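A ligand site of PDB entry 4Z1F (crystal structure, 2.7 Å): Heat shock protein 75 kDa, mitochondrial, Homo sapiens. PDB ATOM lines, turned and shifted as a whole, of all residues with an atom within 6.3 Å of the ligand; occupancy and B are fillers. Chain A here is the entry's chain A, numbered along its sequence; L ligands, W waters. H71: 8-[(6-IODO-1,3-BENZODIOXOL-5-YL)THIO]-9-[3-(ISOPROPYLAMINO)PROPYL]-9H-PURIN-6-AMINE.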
ATOM      1  N   LEU A  57     -14.102   3.202 -34.870  1.00  0.00           N
ATOM      2  CA  LEU A  57     -14.876   2.985 -33.653  1.00  0.00           C
ATOM      3  C   LEU A  57     -13.989   2.582 -32.485  1.00  0.00           C
ATOM      4  O   LEU A  57     -14.294   2.888 -31.337  1.00  0.00           O
ATOM      5  CB  LEU A  57     -15.950   1.910 -33.878  1.00  0.00           C
ATOM      6  CG  LEU A  57     -17.076   2.277 -34.837  1.00  0.00           C
ATOM      7  CD1 LEU A  57     -18.078   1.138 -34.937  1.00  0.00           C
ATOM      8  CD2 LEU A  57     -17.767   3.569 -34.391  1.00  0.00           C
ATOM      9  N   ASN A  60     -12.149   5.973 -31.288  1.00  0.00           N
ATOM     10  CA  ASN A  60     -13.093   6.681 -30.437  1.00  0.00           C
ATOM     11  C   ASN A  60     -13.176   6.062 -29.057  1.00  0.00           C
ATOM     12  O   ASN A  60     -13.031   6.764 -28.043  1.00  0.00           O
ATOM     13  CB  ASN A  60     -14.481   6.710 -31.073  1.00  0.00           C
ATOM     14  CG  ASN A  60     -14.559   7.672 -32.239  1.00  0.00           C
ATOM     15  OD1 ASN A  60     -13.840   8.675 -32.272  1.00  0.00           O
ATOM     16  ND2 ASN A  60     -15.443   7.382 -33.183  1.00  0.00           N
ATOM     17  N   ALA A  61     -13.366   4.739 -29.010  1.00  0.00           N
ATOM     18  CA  ALA A  61     -13.479   4.022 -27.753  1.00  0.00           C
ATOM     19  C   ALA A  61     -12.279   4.376 -26.881  1.00  0.00           C
ATOM     20  O   ALA A  61     -12.442   4.873 -25.766  1.00  0.00           O
ATOM     21  CB  ALA A  61     -13.569   2.528 -27.985  1.00  0.00           C
ATOM     22  N   ALA A  64     -12.388   7.851 -25.506  1.00  0.00           N
ATOM     23  CA  ALA A  64     -13.340   7.945 -24.410  1.00  0.00           C
ATOM     24  C   ALA A  64     -12.649   7.509 -23.143  1.00  0.00           C
ATOM     25  O   ALA A  64     -12.510   8.275 -22.178  1.00  0.00           O
ATOM     26  CB  ALA A  64     -14.571   7.096 -24.691  1.00  0.00           C
ATOM     27  N   LEU A  65     -12.134   6.277 -23.194  1.00  0.00           N
ATOM     28  CA  LEU A  65     -11.490   5.674 -22.039  1.00  0.00           C
ATOM     29  C   LEU A  65     -10.427   6.605 -21.487  1.00  0.00           C
ATOM     30  O   LEU A  65     -10.400   6.875 -20.288  1.00  0.00           O
ATOM     31  CB  LEU A  65     -10.901   4.316 -22.400  1.00  0.00           C
ATOM     32  CG  LEU A  65     -11.935   3.199 -22.376  1.00  0.00           C
ATOM     33  CD1 LEU A  65     -11.401   1.953 -23.035  1.00  0.00           C
ATOM     34  CD2 LEU A  65     -12.360   2.906 -20.941  1.00  0.00           C
ATOM     35  N   ASP A  99     -17.489   0.402 -24.941  1.00  0.00           N
ATOM     36  CA  ASP A  99     -16.385   0.840 -24.101  1.00  0.00           C
ATOM     37  C   ASP A  99     -16.931   1.371 -22.778  1.00  0.00           C
ATOM     38  O   ASP A  99     -18.019   1.958 -22.735  1.00  0.00           O
ATOM     39  CB  ASP A  99     -15.552   1.906 -24.798  1.00  0.00           C
ATOM     40  CG  ASP A  99     -16.332   3.183 -25.051  1.00  0.00           C
ATOM     41  OD1 ASP A  99     -16.423   4.025 -24.132  1.00  0.00           O
ATOM     42  OD2 ASP A  99     -16.837   3.355 -26.181  1.00  0.00           O
ATOM     43  N   GLY A 101     -15.760   3.814 -21.109  1.00  0.00           N
ATOM     44  CA  GLY A 101     -15.118   5.101 -20.963  1.00  0.00           C
ATOM     45  C   GLY A 101     -16.076   6.188 -20.538  1.00  0.00           C
ATOM     46  O   GLY A 101     -17.154   5.909 -20.009  1.00  0.00           O
ATOM     47  N   ILE A 102     -15.680   7.438 -20.748  1.00  0.00           N
ATOM     48  CA  ILE A 102     -16.576   8.550 -20.538  1.00  0.00           C
ATOM     49  C   ILE A 102     -17.672   8.407 -21.592  1.00  0.00           C
ATOM     50  O   ILE A 102     -17.420   7.942 -22.707  1.00  0.00           O
ATOM     51  CB  ILE A 102     -15.853   9.913 -20.635  1.00  0.00           C
ATOM     52  CG1 ILE A 102     -16.233  10.805 -19.451  1.00  0.00           C
ATOM     53  CG2 ILE A 102     -16.151  10.627 -21.952  1.00  0.00           C
ATOM     54  CD1 ILE A 102     -15.465  12.114 -19.391  1.00  0.00           C
ATOM     55  N   GLY A 103     -18.894   8.762 -21.231  1.00  0.00           N
ATOM     56  CA  GLY A 103     -20.019   8.541 -22.122  1.00  0.00           C
ATOM     57  C   GLY A 103     -20.346   9.757 -22.941  1.00  0.00           C
ATOM     58  O   GLY A 103     -19.486  10.609 -23.211  1.00  0.00           O
ATOM     59  N   MET A 104     -21.607   9.852 -23.340  1.00  0.00           N
ATOM     60  CA  MET A 104     -22.103  11.019 -24.039  1.00  0.00           C
ATOM     61  C   MET A 104     -23.367  11.527 -23.350  1.00  0.00           C
ATOM     62  O   MET A 104     -24.290  10.758 -23.076  1.00  0.00           O
ATOM     63  CB  MET A 104     -22.393  10.692 -25.512  1.00  0.00           C
ATOM     64  CG  MET A 104     -21.151  10.563 -26.373  1.00  0.00           C
ATOM     65  SD  MET A 104     -21.519  10.023 -28.057  1.00  0.00           S
ATOM     66  CE  MET A 104     -21.931   8.304 -27.779  1.00  0.00           C
ATOM     67  N   GLU A 108     -24.606  16.118 -26.096  1.00  0.00           N
ATOM     68  CA  GLU A 108     -23.502  15.591 -26.894  1.00  0.00           C
ATOM     69  C   GLU A 108     -23.996  14.642 -27.979  1.00  0.00           C
ATOM     70  O   GLU A 108     -23.365  14.500 -29.029  1.00  0.00           O
ATOM     71  CB  GLU A 108     -22.491  14.889 -25.990  1.00  0.00           C
ATOM     72  CG  GLU A 108     -21.506  15.837 -25.317  1.00  0.00           C
ATOM     73  CD  GLU A 108     -20.843  15.225 -24.099  1.00  0.00           C
ATOM     74  OE1 GLU A 108     -21.159  14.063 -23.768  1.00  0.00           O
ATOM     75  OE2 GLU A 108     -20.000  15.904 -23.485  1.00  0.00           O
ATOM     76  N   LEU A 109     -25.123  13.983 -27.721  1.00  0.00           N
ATOM     77  CA  LEU A 109     -25.732  13.094 -28.703  1.00  0.00           C
ATOM     78  C   LEU A 109     -26.536  13.884 -29.734  1.00  0.00           C
ATOM     79  O   LEU A 109     -26.393  13.658 -30.936  1.00  0.00           O
ATOM     80  CB  LEU A 109     -26.641  12.080 -28.011  1.00  0.00           C
ATOM     81  CG  LEU A 109     -25.933  10.879 -27.361  1.00  0.00           C
ATOM     82  CD1 LEU A 109     -26.831  10.228 -26.327  1.00  0.00           C
ATOM     83  CD2 LEU A 109     -25.519   9.880 -28.424  1.00  0.00           C
ATOM     84  N   ASN A 112     -23.447  16.754 -31.889  1.00  0.00           N
ATOM     85  CA  ASN A 112     -22.520  15.950 -32.677  1.00  0.00           C
ATOM     86  C   ASN A 112     -22.911  14.478 -32.707  1.00  0.00           C
ATOM     87  O   ASN A 112     -24.055  14.139 -33.014  1.00  0.00           O
ATOM     88  CB  ASN A 112     -21.095  16.094 -32.119  1.00  0.00           C
ATOM     89  CG  ASN A 112     -21.014  15.797 -30.634  1.00  0.00           C
ATOM     90  OD1 ASN A 112     -21.135  16.700 -29.802  1.00  0.00           O
ATOM     91  ND2 ASN A 112     -20.800  14.529 -30.288  1.00  0.00           N
ATOM     92  N   GLY A 143     -15.141  13.204 -33.604  1.00  0.00           N
ATOM     93  CA  GLY A 143     -15.358  11.763 -33.635  1.00  0.00           C
ATOM     94  C   GLY A 143     -16.063  11.312 -34.901  1.00  0.00           C
ATOM     95  O   GLY A 143     -16.763  10.302 -34.900  1.00  0.00           O
ATOM     96  N   VAL A 144     -15.856  12.068 -35.971  1.00  0.00           N
ATOM     97  CA  VAL A 144     -16.509  11.825 -37.263  1.00  0.00           C
ATOM     98  C   VAL A 144     -16.293  10.402 -37.786  1.00  0.00           C
ATOM     99  O   VAL A 144     -17.127   9.884 -38.543  1.00  0.00           O
ATOM    100  CB  VAL A 144     -16.012  12.845 -38.312  1.00  0.00           C
ATOM    101  CG1 VAL A 144     -16.725  12.667 -39.648  1.00  0.00           C
ATOM    102  CG2 VAL A 144     -16.207  14.267 -37.802  1.00  0.00           C
ATOM    103  N   GLY A 145     -15.205   9.772 -37.365  1.00  0.00           N
ATOM    104  CA  GLY A 145     -14.918   8.387 -37.730  1.00  0.00           C
ATOM    105  C   GLY A 145     -16.100   7.458 -37.501  1.00  0.00           C
ATOM    106  O   GLY A 145     -16.303   6.500 -38.243  1.00  0.00           O
ATOM    107  N   PHE A 146     -16.879   7.769 -36.461  1.00  0.00           N
ATOM    108  CA  PHE A 146     -18.116   7.049 -36.149  1.00  0.00           C
ATOM    109  C   PHE A 146     -19.003   6.813 -37.360  1.00  0.00           C
ATOM    110  O   PHE A 146     -19.527   5.711 -37.555  1.00  0.00           O
ATOM    111  CB  PHE A 146     -18.896   7.810 -35.083  1.00  0.00           C
ATOM    112  CG  PHE A 146     -20.304   7.311 -34.888  1.00  0.00           C
ATOM    113  CD1 PHE A 146     -20.556   6.160 -34.158  1.00  0.00           C
ATOM    114  CD2 PHE A 146     -21.385   8.013 -35.415  1.00  0.00           C
ATOM    115  CE1 PHE A 146     -21.851   5.700 -33.979  1.00  0.00           C
ATOM    116  CE2 PHE A 146     -22.677   7.562 -35.239  1.00  0.00           C
ATOM    117  CZ  PHE A 146     -22.912   6.401 -34.519  1.00  0.00           C
ATOM    118  N   TYR A 147     -19.178   7.845 -38.177  1.00  0.00           N
ATOM    119  CA  TYR A 147     -20.107   7.769 -39.304  1.00  0.00           C
ATOM    120  C   TYR A 147     -19.662   6.768 -40.371  1.00  0.00           C
ATOM    121  O   TYR A 147     -20.458   6.372 -41.221  1.00  0.00           O
ATOM    122  CB  TYR A 147     -20.296   9.159 -39.920  1.00  0.00           C
ATOM    123  CG  TYR A 147     -21.049  10.096 -39.005  1.00  0.00           C
ATOM    124  CD1 TYR A 147     -20.406  11.132 -38.344  1.00  0.00           C
ATOM    125  CD2 TYR A 147     -22.404   9.915 -38.774  1.00  0.00           C
ATOM    126  CE1 TYR A 147     -21.097  11.986 -37.496  1.00  0.00           C
ATOM    127  CE2 TYR A 147     -23.108  10.761 -37.932  1.00  0.00           C
ATOM    128  CZ  TYR A 147     -22.446  11.793 -37.294  1.00  0.00           C
ATOM    129  OH  TYR A 147     -23.132  12.631 -36.452  1.00  0.00           O
ATOM    130  N   VAL A 158     -27.284   2.926 -30.861  1.00  0.00           N
ATOM    131  CA  VAL A 158     -26.318   3.364 -29.856  1.00  0.00           C
ATOM    132  C   VAL A 158     -26.951   3.520 -28.474  1.00  0.00           C
ATOM    133  O   VAL A 158     -28.063   4.020 -28.349  1.00  0.00           O
ATOM    134  CB  VAL A 158     -25.679   4.716 -30.275  1.00  0.00           C
ATOM    135  CG1 VAL A 158     -24.646   5.158 -29.248  1.00  0.00           C
ATOM    136  CG2 VAL A 158     -25.048   4.609 -31.650  1.00  0.00           C
ATOM    137  N   SER A 160     -25.674   5.178 -24.769  1.00  0.00           N
ATOM    138  CA  SER A 160     -24.570   5.888 -24.125  1.00  0.00           C
ATOM    139  C   SER A 160     -24.995   6.558 -22.817  1.00  0.00           C
ATOM    140  O   SER A 160     -26.128   7.005 -22.674  1.00  0.00           O
ATOM    141  CB  SER A 160     -23.985   6.934 -25.067  1.00  0.00           C
ATOM    142  OG  SER A 160     -22.837   7.541 -24.504  1.00  0.00           O
ATOM    143  N   TRP A 172     -29.852   6.128 -29.166  1.00  0.00           N
ATOM    144  CA  TRP A 172     -29.711   6.886 -30.406  1.00  0.00           C
ATOM    145  C   TRP A 172     -29.864   5.930 -31.575  1.00  0.00           C
ATOM    146  O   TRP A 172     -29.155   4.938 -31.660  1.00  0.00           O
ATOM    147  CB  TRP A 172     -28.352   7.578 -30.431  1.00  0.00           C
ATOM    148  CG  TRP A 172     -28.074   8.434 -31.624  1.00  0.00           C
ATOM    149  CD1 TRP A 172     -28.215   9.795 -31.712  1.00  0.00           C
ATOM    150  CD2 TRP A 172     -27.585   8.000 -32.895  1.00  0.00           C
ATOM    151  NE1 TRP A 172     -27.851  10.224 -32.958  1.00  0.00           N
ATOM    152  CE2 TRP A 172     -27.455   9.147 -33.712  1.00  0.00           C
ATOM    153  CE3 TRP A 172     -27.233   6.754 -33.435  1.00  0.00           C
ATOM    154  CZ2 TRP A 172     -26.999   9.085 -35.025  1.00  0.00           C
ATOM    155  CZ3 TRP A 172     -26.776   6.696 -34.739  1.00  0.00           C
ATOM    156  CH2 TRP A 172     -26.663   7.852 -35.515  1.00  0.00           C
ATOM    157  N   GLY A 191     -20.410   4.668 -20.267  1.00  0.00           N
ATOM    158  CA  GLY A 191     -19.647   4.430 -21.473  1.00  0.00           C
ATOM    159  C   GLY A 191     -20.574   4.360 -22.676  1.00  0.00           C
ATOM    160  O   GLY A 191     -21.696   4.865 -22.615  1.00  0.00           O
ATOM    161  N   THR A 192     -20.121   3.727 -23.747  1.00  0.00           N
ATOM    162  CA  THR A 192     -20.903   3.723 -24.988  1.00  0.00           C
ATOM    163  C   THR A 192     -20.985   2.340 -25.610  1.00  0.00           C
ATOM    164  O   THR A 192     -19.988   1.634 -25.711  1.00  0.00           O
ATOM    165  CB  THR A 192     -20.310   4.712 -26.019  1.00  0.00           C
ATOM    166  OG1 THR A 192     -20.318   6.036 -25.474  1.00  0.00           O
ATOM    167  CG2 THR A 192     -21.121   4.692 -27.305  1.00  0.00           C
ATOM    168  N   ILE A 194     -22.195   0.551 -29.158  1.00  0.00           N
ATOM    169  CA  ILE A 194     -22.625   0.753 -30.538  1.00  0.00           C
ATOM    170  C   ILE A 194     -22.966  -0.575 -31.205  1.00  0.00           C
ATOM    171  O   ILE A 194     -22.091  -1.419 -31.418  1.00  0.00           O
ATOM    172  CB  ILE A 194     -21.548   1.469 -31.374  1.00  0.00           C
ATOM    173  CG1 ILE A 194     -21.224   2.836 -30.779  1.00  0.00           C
ATOM    174  CG2 ILE A 194     -22.015   1.609 -32.814  1.00  0.00           C
ATOM    175  CD1 ILE A 194     -20.100   3.555 -31.485  1.00  0.00           C
HETATM  176  C96 H71 L   1     -17.423  12.885 -25.130  1.00  0.00           C
HETATM  177  C95 H71 L   1     -17.768  13.432 -26.496  1.00  0.00           C
HETATM  178  C97 H71 L   1     -18.127  14.886 -26.373  1.00  0.00           C
HETATM  179  N94 H71 L   1     -16.628  13.290 -27.382  1.00  0.00           N
HETATM  180  C93 H71 L   1     -17.002  13.633 -28.747  1.00  0.00           C
HETATM  181  C92 H71 L   1     -16.934  12.387 -29.618  1.00  0.00           C
HETATM  182  C91 H71 L   1     -18.291  11.701 -29.606  1.00  0.00           C
HETATM  183  N9  H71 L   1     -18.108  10.253 -29.392  1.00  0.00           N
HETATM  184  C4  H71 L   1     -17.900   9.582 -28.118  1.00  0.00           C
HETATM  185  N3  H71 L   1     -17.810  10.007 -26.858  1.00  0.00           N
HETATM  186  C2  H71 L   1     -17.601   9.133 -25.840  1.00  0.00           C
HETATM  187  N1  H71 L   1     -17.478   7.793 -26.070  1.00  0.00           N
HETATM  188  C6  H71 L   1     -17.558   7.313 -27.316  1.00  0.00           C
HETATM  189  N6  H71 L   1     -17.422   5.896 -27.557  1.00  0.00           N
HETATM  190  C5  H71 L   1     -17.769   8.181 -28.384  1.00  0.00           C
HETATM  191  N7  H71 L   1     -17.914   7.999 -29.825  1.00  0.00           N
HETATM  192  C8  H71 L   1     -18.099   9.267 -30.395  1.00  0.00           C
HETATM  193  S   H71 L   1     -18.334   9.589 -32.119  1.00  0.00           S
HETATM  194  C1' H71 L   1     -20.077   9.819 -32.294  1.00  0.00           C
HETATM  195  C6' H71 L   1     -20.910   8.814 -31.847  1.00  0.00           C
HETATM  196  C5' H71 L   1     -22.292   8.948 -31.946  1.00  0.00           C
HETATM  197  O3' H71 L   1     -23.317   8.111 -31.596  1.00  0.00           O
HETATM  198  C'2 H71 L   1     -24.441   8.630 -32.211  1.00  0.00           C
HETATM  199  O1' H71 L   1     -24.185   9.965 -32.471  1.00  0.00           O
HETATM  200  C4' H71 L   1     -22.827  10.095 -32.487  1.00  0.00           C
HETATM  201  C3' H71 L   1     -21.986  11.120 -32.932  1.00  0.00           C
HETATM  202  C2' H71 L   1     -20.604  10.986 -32.832  1.00  0.00           C
HETATM  203  I   H71 L   1     -19.339  12.532 -33.506  1.00  0.00           I
HETATM  204  O   HOH W   1     -17.556   6.182 -32.132  1.00  0.00           O
HETATM  205  O   HOH W   2     -17.581  14.996 -32.204  1.00  0.00           O
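A nitrogen (N1) of the ligand sits at hydrogen-bond distance from the side-chain hydroxyl (OG1) of Thr 192.
A sulfur (S) of the ligand lies close to the side-chain amide nitrogen (ND2) of Asn 60 (3.8 Å).
A nitrogen (N6) of the ligand sits at hydrogen-bond distance from the side-chain carboxylate (OD2) of Asp 99, at 2.9 Å.
The side-chain hydroxyl of Ser 160 sits at hydrogen-bond distance from the side-chain hydroxyl of Thr 192.
ND2 of Asn 112 lies within hydrogen-bond range of O of Glu 108, 2.9 Å away.
O of Thr 192 lies within hydrogen-bond range of N of Asp 99, at 2.9 Å.
N of Met 104 sits at hydrogen-bond distance from OG of Ser 160 (2.9 Å).
OD1 of Asp 99 lies within hydrogen-bond range of N of Gly 101, at 3.1 Å.
O of Trp 172 lies within hydrogen-bond range of N of Val 158, at 2.9 Å.
O of Ile 102 lies close to N1 of the ligand (3.4 Å).
The side-chain sulfur (SD) of Met 104 sits close to a nitrogen (N9) of the ligand.
The backbone carbonyl oxygen (O) of Gly 143 sits close to a sulfur (S) of the ligand, 3.3 Å away.
Residues that only touch the ligand: Trp 172, Ala 64, Phe 146, Asn 112, Gly 103, Glu 108, Val 158 and Tyr 147.
Water W1 lies within hydrogen-bond range of ND2 of Asn 60 and N7 of the ligand.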
